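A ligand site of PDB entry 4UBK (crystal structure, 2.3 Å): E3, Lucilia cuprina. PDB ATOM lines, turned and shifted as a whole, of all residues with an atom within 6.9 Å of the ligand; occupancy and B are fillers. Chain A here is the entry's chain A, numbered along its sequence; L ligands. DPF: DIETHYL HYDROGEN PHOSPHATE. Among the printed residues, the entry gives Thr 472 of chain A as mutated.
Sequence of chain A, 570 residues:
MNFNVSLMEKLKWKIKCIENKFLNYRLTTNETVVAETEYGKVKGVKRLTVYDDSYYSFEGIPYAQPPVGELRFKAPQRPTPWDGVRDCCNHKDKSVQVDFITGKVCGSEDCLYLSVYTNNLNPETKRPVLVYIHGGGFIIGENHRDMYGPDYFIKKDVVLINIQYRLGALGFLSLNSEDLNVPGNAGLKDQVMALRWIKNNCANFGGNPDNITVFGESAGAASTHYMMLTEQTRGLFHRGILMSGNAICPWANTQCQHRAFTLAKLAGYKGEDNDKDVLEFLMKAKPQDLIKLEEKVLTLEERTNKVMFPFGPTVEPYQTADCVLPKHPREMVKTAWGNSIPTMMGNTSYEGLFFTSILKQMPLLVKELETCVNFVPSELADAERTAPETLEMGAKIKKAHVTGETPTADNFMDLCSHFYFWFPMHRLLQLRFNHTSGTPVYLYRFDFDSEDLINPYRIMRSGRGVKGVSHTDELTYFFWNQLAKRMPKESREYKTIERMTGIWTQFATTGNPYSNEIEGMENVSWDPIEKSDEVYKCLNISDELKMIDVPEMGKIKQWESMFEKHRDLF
A phosphorus (P1) of the ligand is bonded to the side-chain hydroxyl (OG) of Ser 218 (1.5 Å).
The backbone NH (N) of Ala 219 is in hydrogen-bond range of an oxygen (O4) of the ligand, at 2.7 Å.
O4 of the ligand lies within hydrogen-bond range of N of Gly 137.
An oxygen (O4) of the ligand lies within hydrogen-bond range of the backbone NH of Gly 136 (2.9 Å).
The backbone NH (N) of Ser 218 lies close to the backbone carbonyl oxygen (O) of Ser 244, at 3.5 Å.
The side-chain hydroxyl (OG) of Ser 218 lies within hydrogen-bond range of a ring nitrogen (NE2) of His 471.
A ring nitrogen (NE2) of His 471 lies within hydrogen-bond range of the side-chain carboxylate of Glu 217, 2.9 Å away.
The indole nitrogen of Trp 251 lies within hydrogen-bond range of the backbone carbonyl oxygen of Tyr 420 (3.0 Å).
Gly 135 touches the ligand (C to O4, 3.9 Å).
Trp 251 touches the ligand (CD2 to C1, 3.6 Å).
Met 308 touches the ligand.
Phe 354 touches the ligand (CZ to C3, 3.5 Å).
Tyr 457 touches the ligand.
NE2 of His 471 touches C2 of the ligand, 3.5 Å away.
Thr 472 touches the ligand (CG2 to C3, 3.6 Å).
Within 4 Å of the ligand: Gly 135, Gly 136, Gly 137, Ser 218, Ala 219, Trp 251, Met 308, Phe 354, Tyr 457, His 471 and Thr 472.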
ATOM      1  N   HIS A 134       2.337 -15.109   2.418  1.00  0.00           N
ATOM      2  CA  HIS A 134       1.690 -13.824   2.138  1.00  0.00           C
ATOM      3  C   HIS A 134       2.667 -12.865   1.486  1.00  0.00           C
ATOM      4  O   HIS A 134       3.888 -13.037   1.575  1.00  0.00           O
ATOM      5  CB  HIS A 134       1.113 -13.221   3.418  1.00  0.00           C
ATOM      6  CG  HIS A 134       2.161 -12.796   4.398  1.00  0.00           C
ATOM      7  ND1 HIS A 134       2.796 -11.566   4.325  1.00  0.00           N
ATOM      8  CD2 HIS A 134       2.698 -13.422   5.470  1.00  0.00           C
ATOM      9  CE1 HIS A 134       3.667 -11.463   5.306  1.00  0.00           C
ATOM     10  NE2 HIS A 134       3.632 -12.573   6.010  1.00  0.00           N
ATOM     11  N   GLY A 135       2.104 -11.862   0.798  1.00  0.00           N
ATOM     12  CA  GLY A 135       2.868 -10.822   0.154  1.00  0.00           C
ATOM     13  C   GLY A 135       2.860  -9.618   1.059  1.00  0.00           C
ATOM     14  O   GLY A 135       2.459  -9.732   2.226  1.00  0.00           O
ATOM     15  N   GLY A 136       3.274  -8.478   0.542  1.00  0.00           N
ATOM     16  CA  GLY A 136       3.379  -7.270   1.333  1.00  0.00           C
ATOM     17  C   GLY A 136       4.752  -6.636   1.216  1.00  0.00           C
ATOM     18  O   GLY A 136       5.262  -6.026   2.172  1.00  0.00           O
ATOM     19  N   GLY A 137       5.351  -6.792   0.034  1.00  0.00           N
ATOM     20  CA  GLY A 137       6.640  -6.203  -0.281  1.00  0.00           C
ATOM     21  C   GLY A 137       7.738  -6.497   0.733  1.00  0.00           C
ATOM     22  O   GLY A 137       8.680  -5.697   0.857  1.00  0.00           O
ATOM     23  N   PHE A 138       7.615  -7.612   1.451  1.00  0.00           N
ATOM     24  CA  PHE A 138       8.531  -7.983   2.542  1.00  0.00           C
ATOM     25  C   PHE A 138       8.553  -6.978   3.709  1.00  0.00           C
ATOM     26  O   PHE A 138       9.422  -7.049   4.577  1.00  0.00           O
ATOM     27  CB  PHE A 138       9.959  -8.185   1.995  1.00  0.00           C
ATOM     28  CG  PHE A 138      10.052  -9.206   0.885  1.00  0.00           C
ATOM     29  CD1 PHE A 138      10.065 -10.562   1.171  1.00  0.00           C
ATOM     30  CD2 PHE A 138      10.130  -8.801  -0.443  1.00  0.00           C
ATOM     31  CE1 PHE A 138      10.137 -11.498   0.137  1.00  0.00           C
ATOM     32  CE2 PHE A 138      10.211  -9.732  -1.479  1.00  0.00           C
ATOM     33  CZ  PHE A 138      10.219 -11.077  -1.186  1.00  0.00           C
ATOM     34  N   ILE A 140       5.151  -5.660   5.040  1.00  0.00           N
ATOM     35  CA  ILE A 140       3.883  -5.830   5.770  1.00  0.00           C
ATOM     36  C   ILE A 140       3.302  -7.202   5.469  1.00  0.00           C
ATOM     37  O   ILE A 140       3.786  -7.923   4.575  1.00  0.00           O
ATOM     38  CB  ILE A 140       2.805  -4.789   5.419  1.00  0.00           C
ATOM     39  CG1 ILE A 140       2.351  -4.954   3.960  1.00  0.00           C
ATOM     40  CG2 ILE A 140       3.255  -3.370   5.762  1.00  0.00           C
ATOM     41  CD1 ILE A 140       1.212  -4.037   3.547  1.00  0.00           C
ATOM     42  N   GLU A 217       1.268 -14.555  -3.305  1.00  0.00           N
ATOM     43  CA  GLU A 217       0.989 -13.428  -4.180  1.00  0.00           C
ATOM     44  C   GLU A 217       1.968 -12.247  -3.921  1.00  0.00           C
ATOM     45  O   GLU A 217       2.350 -11.992  -2.781  1.00  0.00           O
ATOM     46  CB  GLU A 217      -0.481 -13.002  -3.989  1.00  0.00           C
ATOM     47  CG  GLU A 217      -0.982 -11.915  -4.905  1.00  0.00           C
ATOM     48  CD  GLU A 217      -0.920 -10.555  -4.257  1.00  0.00           C
ATOM     49  OE1 GLU A 217      -0.824 -10.487  -3.004  1.00  0.00           O
ATOM     50  OE2 GLU A 217      -0.957  -9.534  -5.002  1.00  0.00           O
ATOM     51  N   SER A 218       2.387 -11.575  -4.989  1.00  0.00           N
ATOM     52  CA  SER A 218       3.319 -10.437  -4.923  1.00  0.00           C
ATOM     53  C   SER A 218       4.662 -10.861  -4.303  1.00  0.00           C
ATOM     54  O   SER A 218       5.329 -11.736  -4.844  1.00  0.00           O
ATOM     55  CB  SER A 218       2.684  -9.286  -4.129  1.00  0.00           C
ATOM     56  OG  SER A 218       3.248  -8.030  -4.485  1.00  0.00           O
ATOM     57  N   ALA A 219       5.025 -10.255  -3.162  1.00  0.00           N
ATOM     58  CA  ALA A 219       6.220 -10.682  -2.424  1.00  0.00           C
ATOM     59  C   ALA A 219       6.130 -12.152  -2.034  1.00  0.00           C
ATOM     60  O   ALA A 219       7.149 -12.822  -1.890  1.00  0.00           O
ATOM     61  CB  ALA A 219       6.416  -9.818  -1.169  1.00  0.00           C
ATOM     62  N   GLY A 220       4.913 -12.660  -1.859  1.00  0.00           N
ATOM     63  CA  GLY A 220       4.721 -14.059  -1.538  1.00  0.00           C
ATOM     64  C   GLY A 220       5.053 -14.948  -2.713  1.00  0.00           C
ATOM     65  O   GLY A 220       5.561 -16.063  -2.548  1.00  0.00           O
ATOM     66  N   ALA A 221       4.769 -14.464  -3.914  1.00  0.00           N
ATOM     67  CA  ALA A 221       5.134 -15.178  -5.121  1.00  0.00           C
ATOM     68  C   ALA A 221       6.669 -15.208  -5.274  1.00  0.00           C
ATOM     69  O   ALA A 221       7.257 -16.232  -5.635  1.00  0.00           O
ATOM     70  CB  ALA A 221       4.477 -14.516  -6.333  1.00  0.00           C
ATOM     71  N   SER A 244       1.235 -13.221  -9.537  1.00  0.00           N
ATOM     72  CA  SER A 244       1.696 -11.845  -9.722  1.00  0.00           C
ATOM     73  C   SER A 244       3.062 -11.613  -9.099  1.00  0.00           C
ATOM     74  O   SER A 244       3.225 -10.726  -8.262  1.00  0.00           O
ATOM     75  CB  SER A 244       0.711 -10.820  -9.122  1.00  0.00           C
ATOM     76  OG  SER A 244      -0.581 -10.928  -9.708  1.00  0.00           O
ATOM     77  N   TRP A 251      11.586  -5.439  -8.046  1.00  0.00           N
ATOM     78  CA  TRP A 251      11.335  -5.137  -6.645  1.00  0.00           C
ATOM     79  C   TRP A 251      11.655  -6.295  -5.676  1.00  0.00           C
ATOM     80  O   TRP A 251      11.494  -6.139  -4.456  1.00  0.00           O
ATOM     81  CB  TRP A 251       9.860  -4.732  -6.467  1.00  0.00           C
ATOM     82  CG  TRP A 251       8.916  -5.693  -7.146  1.00  0.00           C
ATOM     83  CD1 TRP A 251       8.401  -5.593  -8.421  1.00  0.00           C
ATOM     84  CD2 TRP A 251       8.390  -6.915  -6.602  1.00  0.00           C
ATOM     85  NE1 TRP A 251       7.591  -6.673  -8.690  1.00  0.00           N
ATOM     86  CE2 TRP A 251       7.559  -7.494  -7.592  1.00  0.00           C
ATOM     87  CE3 TRP A 251       8.531  -7.576  -5.375  1.00  0.00           C
ATOM     88  CZ2 TRP A 251       6.898  -8.703  -7.394  1.00  0.00           C
ATOM     89  CZ3 TRP A 251       7.851  -8.774  -5.178  1.00  0.00           C
ATOM     90  CH2 TRP A 251       7.047  -9.326  -6.183  1.00  0.00           C
ATOM     91  N   MET A 308      12.210   0.148  -4.770  1.00  0.00           N
ATOM     92  CA  MET A 308      10.904   0.263  -4.129  1.00  0.00           C
ATOM     93  C   MET A 308      10.986   0.131  -2.597  1.00  0.00           C
ATOM     94  O   MET A 308      10.255   0.793  -1.874  1.00  0.00           O
ATOM     95  CB  MET A 308       9.951  -0.782  -4.729  1.00  0.00           C
ATOM     96  CG  MET A 308       8.572  -0.818  -4.092  1.00  0.00           C
ATOM     97  SD  MET A 308       7.421  -1.880  -4.996  1.00  0.00           S
ATOM     98  CE  MET A 308       7.135  -0.864  -6.456  1.00  0.00           C
ATOM     99  N   PHE A 309      11.886  -0.730  -2.121  1.00  0.00           N
ATOM    100  CA  PHE A 309      12.077  -0.968  -0.691  1.00  0.00           C
ATOM    101  C   PHE A 309      13.564  -0.920  -0.325  1.00  0.00           C
ATOM    102  O   PHE A 309      14.416  -1.400  -1.094  1.00  0.00           O
ATOM    103  CB  PHE A 309      11.493  -2.318  -0.272  1.00  0.00           C
ATOM    104  CG  PHE A 309      10.088  -2.556  -0.746  1.00  0.00           C
ATOM    105  CD1 PHE A 309       9.033  -1.848  -0.204  1.00  0.00           C
ATOM    106  CD2 PHE A 309       9.830  -3.520  -1.702  1.00  0.00           C
ATOM    107  CE1 PHE A 309       7.717  -2.083  -0.627  1.00  0.00           C
ATOM    108  CE2 PHE A 309       8.517  -3.771  -2.140  1.00  0.00           C
ATOM    109  CZ  PHE A 309       7.461  -3.039  -1.597  1.00  0.00           C
ATOM    110  N   PHE A 354      -3.021  -0.820  -9.412  1.00  0.00           N
ATOM    111  CA  PHE A 354      -2.647  -0.706  -8.020  1.00  0.00           C
ATOM    112  C   PHE A 354      -2.048   0.669  -7.668  1.00  0.00           C
ATOM    113  O   PHE A 354      -2.179   1.155  -6.542  1.00  0.00           O
ATOM    114  CB  PHE A 354      -1.666  -1.817  -7.681  1.00  0.00           C
ATOM    115  CG  PHE A 354      -1.319  -1.892  -6.230  1.00  0.00           C
ATOM    116  CD1 PHE A 354      -0.248  -1.196  -5.722  1.00  0.00           C
ATOM    117  CD2 PHE A 354      -2.096  -2.657  -5.358  1.00  0.00           C
ATOM    118  CE1 PHE A 354       0.068  -1.259  -4.369  1.00  0.00           C
ATOM    119  CE2 PHE A 354      -1.781  -2.724  -4.015  1.00  0.00           C
ATOM    120  CZ  PHE A 354      -0.695  -2.023  -3.522  1.00  0.00           C
ATOM    121  N   PHE A 355      -1.393   1.305  -8.645  1.00  0.00           N
ATOM    122  CA  PHE A 355      -0.643   2.529  -8.383  1.00  0.00           C
ATOM    123  C   PHE A 355      -1.459   3.817  -8.522  1.00  0.00           C
ATOM    124  O   PHE A 355      -0.898   4.904  -8.527  1.00  0.00           O
ATOM    125  CB  PHE A 355       0.587   2.603  -9.297  1.00  0.00           C
ATOM    126  CG  PHE A 355       1.549   1.464  -9.086  1.00  0.00           C
ATOM    127  CD1 PHE A 355       2.544   1.543  -8.134  1.00  0.00           C
ATOM    128  CD2 PHE A 355       1.418   0.292  -9.823  1.00  0.00           C
ATOM    129  CE1 PHE A 355       3.410   0.488  -7.922  1.00  0.00           C
ATOM    130  CE2 PHE A 355       2.280  -0.779  -9.615  1.00  0.00           C
ATOM    131  CZ  PHE A 355       3.274  -0.676  -8.661  1.00  0.00           C
ATOM    132  N   TYR A 420       6.761  -4.102 -13.575  1.00  0.00           N
ATOM    133  CA  TYR A 420       6.798  -4.841 -12.325  1.00  0.00           C
ATOM    134  C   TYR A 420       6.364  -6.299 -12.426  1.00  0.00           C
ATOM    135  O   TYR A 420       6.652  -7.087 -11.526  1.00  0.00           O
ATOM    136  CB  TYR A 420       5.918  -4.130 -11.275  1.00  0.00           C
ATOM    137  CG  TYR A 420       6.440  -2.779 -10.871  1.00  0.00           C
ATOM    138  CD1 TYR A 420       7.668  -2.646 -10.221  1.00  0.00           C
ATOM    139  CD2 TYR A 420       5.706  -1.624 -11.130  1.00  0.00           C
ATOM    140  CE1 TYR A 420       8.166  -1.403  -9.824  1.00  0.00           C
ATOM    141  CE2 TYR A 420       6.204  -0.371 -10.748  1.00  0.00           C
ATOM    142  CZ  TYR A 420       7.426  -0.268 -10.096  1.00  0.00           C
ATOM    143  OH  TYR A 420       7.926   0.960  -9.715  1.00  0.00           O
ATOM    144  N   PHE A 421       5.666  -6.675 -13.495  1.00  0.00           N
ATOM    145  CA  PHE A 421       5.068  -8.013 -13.492  1.00  0.00           C
ATOM    146  C   PHE A 421       5.183  -8.815 -14.792  1.00  0.00           C
ATOM    147  O   PHE A 421       5.738  -9.920 -14.779  1.00  0.00           O
ATOM    148  CB  PHE A 421       3.589  -7.909 -13.105  1.00  0.00           C
ATOM    149  CG  PHE A 421       3.360  -7.360 -11.719  1.00  0.00           C
ATOM    150  CD1 PHE A 421       3.655  -8.121 -10.592  1.00  0.00           C
ATOM    151  CD2 PHE A 421       2.846  -6.081 -11.548  1.00  0.00           C
ATOM    152  CE1 PHE A 421       3.454  -7.618  -9.334  1.00  0.00           C
ATOM    153  CE2 PHE A 421       2.639  -5.574 -10.267  1.00  0.00           C
ATOM    154  CZ  PHE A 421       2.939  -6.342  -9.171  1.00  0.00           C
ATOM    155  N   TYR A 457      -6.512  -4.623   0.919  1.00  0.00           N
ATOM    156  CA  TYR A 457      -5.586  -3.957   0.001  1.00  0.00           C
ATOM    157  C   TYR A 457      -6.283  -2.904  -0.874  1.00  0.00           C
ATOM    158  O   TYR A 457      -5.626  -2.000  -1.394  1.00  0.00           O
ATOM    159  CB  TYR A 457      -4.894  -4.968  -0.912  1.00  0.00           C
ATOM    160  CG  TYR A 457      -3.727  -5.677  -0.294  1.00  0.00           C
ATOM    161  CD1 TYR A 457      -2.507  -5.034  -0.122  1.00  0.00           C
ATOM    162  CD2 TYR A 457      -3.822  -7.016   0.087  1.00  0.00           C
ATOM    163  CE1 TYR A 457      -1.424  -5.683   0.429  1.00  0.00           C
ATOM    164  CE2 TYR A 457      -2.741  -7.677   0.643  1.00  0.00           C
ATOM    165  CZ  TYR A 457      -1.537  -7.007   0.817  1.00  0.00           C
ATOM    166  OH  TYR A 457      -0.466  -7.677   1.367  1.00  0.00           O
ATOM    167  N   MET A 460      -5.938   0.532   0.624  1.00  0.00           N
ATOM    168  CA  MET A 460      -4.605   1.112   0.546  1.00  0.00           C
ATOM    169  C   MET A 460      -4.308   1.689  -0.837  1.00  0.00           C
ATOM    170  O   MET A 460      -3.802   2.806  -0.945  1.00  0.00           O
ATOM    171  CB  MET A 460      -3.558   0.060   0.927  1.00  0.00           C
ATOM    172  CG  MET A 460      -2.117   0.501   0.727  1.00  0.00           C
ATOM    173  SD  MET A 460      -0.997  -0.922   0.564  1.00  0.00           S
ATOM    174  CE  MET A 460      -1.558  -1.936   1.931  1.00  0.00           C
ATOM    175  N   HIS A 471      -3.801  -5.566  -9.201  1.00  0.00           N
ATOM    176  CA  HIS A 471      -2.965  -6.364  -8.339  1.00  0.00           C
ATOM    177  C   HIS A 471      -3.652  -6.559  -6.960  1.00  0.00           C
ATOM    178  O   HIS A 471      -4.190  -5.604  -6.404  1.00  0.00           O
ATOM    179  CB  HIS A 471      -1.605  -5.674  -8.205  1.00  0.00           C
ATOM    180  CG  HIS A 471      -0.604  -6.465  -7.444  1.00  0.00           C
ATOM    181  ND1 HIS A 471       0.017  -7.569  -7.974  1.00  0.00           N
ATOM    182  CD2 HIS A 471      -0.154  -6.349  -6.172  1.00  0.00           C
ATOM    183  CE1 HIS A 471       0.832  -8.092  -7.068  1.00  0.00           C
ATOM    184  NE2 HIS A 471       0.740  -7.373  -5.966  1.00  0.00           N
ATOM    185  N   THR A 472      -3.662  -7.801  -6.457  1.00  0.00           N
ATOM    186  CA  THR A 472      -4.343  -8.255  -5.202  1.00  0.00           C
ATOM    187  C   THR A 472      -5.868  -8.394  -5.254  1.00  0.00           C
ATOM    188  O   THR A 472      -6.477  -8.835  -4.275  1.00  0.00           O
ATOM    189  CB  THR A 472      -4.062  -7.337  -3.959  1.00  0.00           C
ATOM    190  OG1 THR A 472      -4.853  -6.140  -4.042  1.00  0.00           O
ATOM    191  CG2 THR A 472      -2.587  -6.997  -3.796  1.00  0.00           C
ATOM    192  N   LEU A 475      -7.156 -12.045  -4.384  1.00  0.00           N
ATOM    193  CA  LEU A 475      -7.049 -12.623  -3.056  1.00  0.00           C
ATOM    194  C   LEU A 475      -8.432 -12.826  -2.460  1.00  0.00           C
ATOM    195  O   LEU A 475      -8.696 -13.822  -1.771  1.00  0.00           O
ATOM    196  CB  LEU A 475      -6.227 -11.730  -2.126  1.00  0.00           C
ATOM    197  CG  LEU A 475      -4.737 -11.649  -2.426  1.00  0.00           C
ATOM    198  CD1 LEU A 475      -4.042 -10.684  -1.465  1.00  0.00           C
ATOM    199  CD2 LEU A 475      -4.088 -13.036  -2.399  1.00  0.00           C
HETATM  200  O4  DPF L   1       4.061  -7.875  -2.201  1.00  0.00           O
HETATM  201  P1  DPF L   1       3.660  -7.055  -3.392  1.00  0.00           P
HETATM  202  O3  DPF L   1       4.932  -6.069  -3.724  1.00  0.00           O
HETATM  203  C1  DPF L   1       5.341  -5.960  -5.042  1.00  0.00           C
HETATM  204  C4  DPF L   1       5.084  -4.533  -5.486  1.00  0.00           C
HETATM  205  O1  DPF L   1       2.529  -5.998  -2.807  1.00  0.00           O
HETATM  206  C2  DPF L   1       1.257  -6.465  -2.619  1.00  0.00           C
HETATM  207  C3  DPF L   1       0.320  -5.279  -2.657  1.00  0.00           C
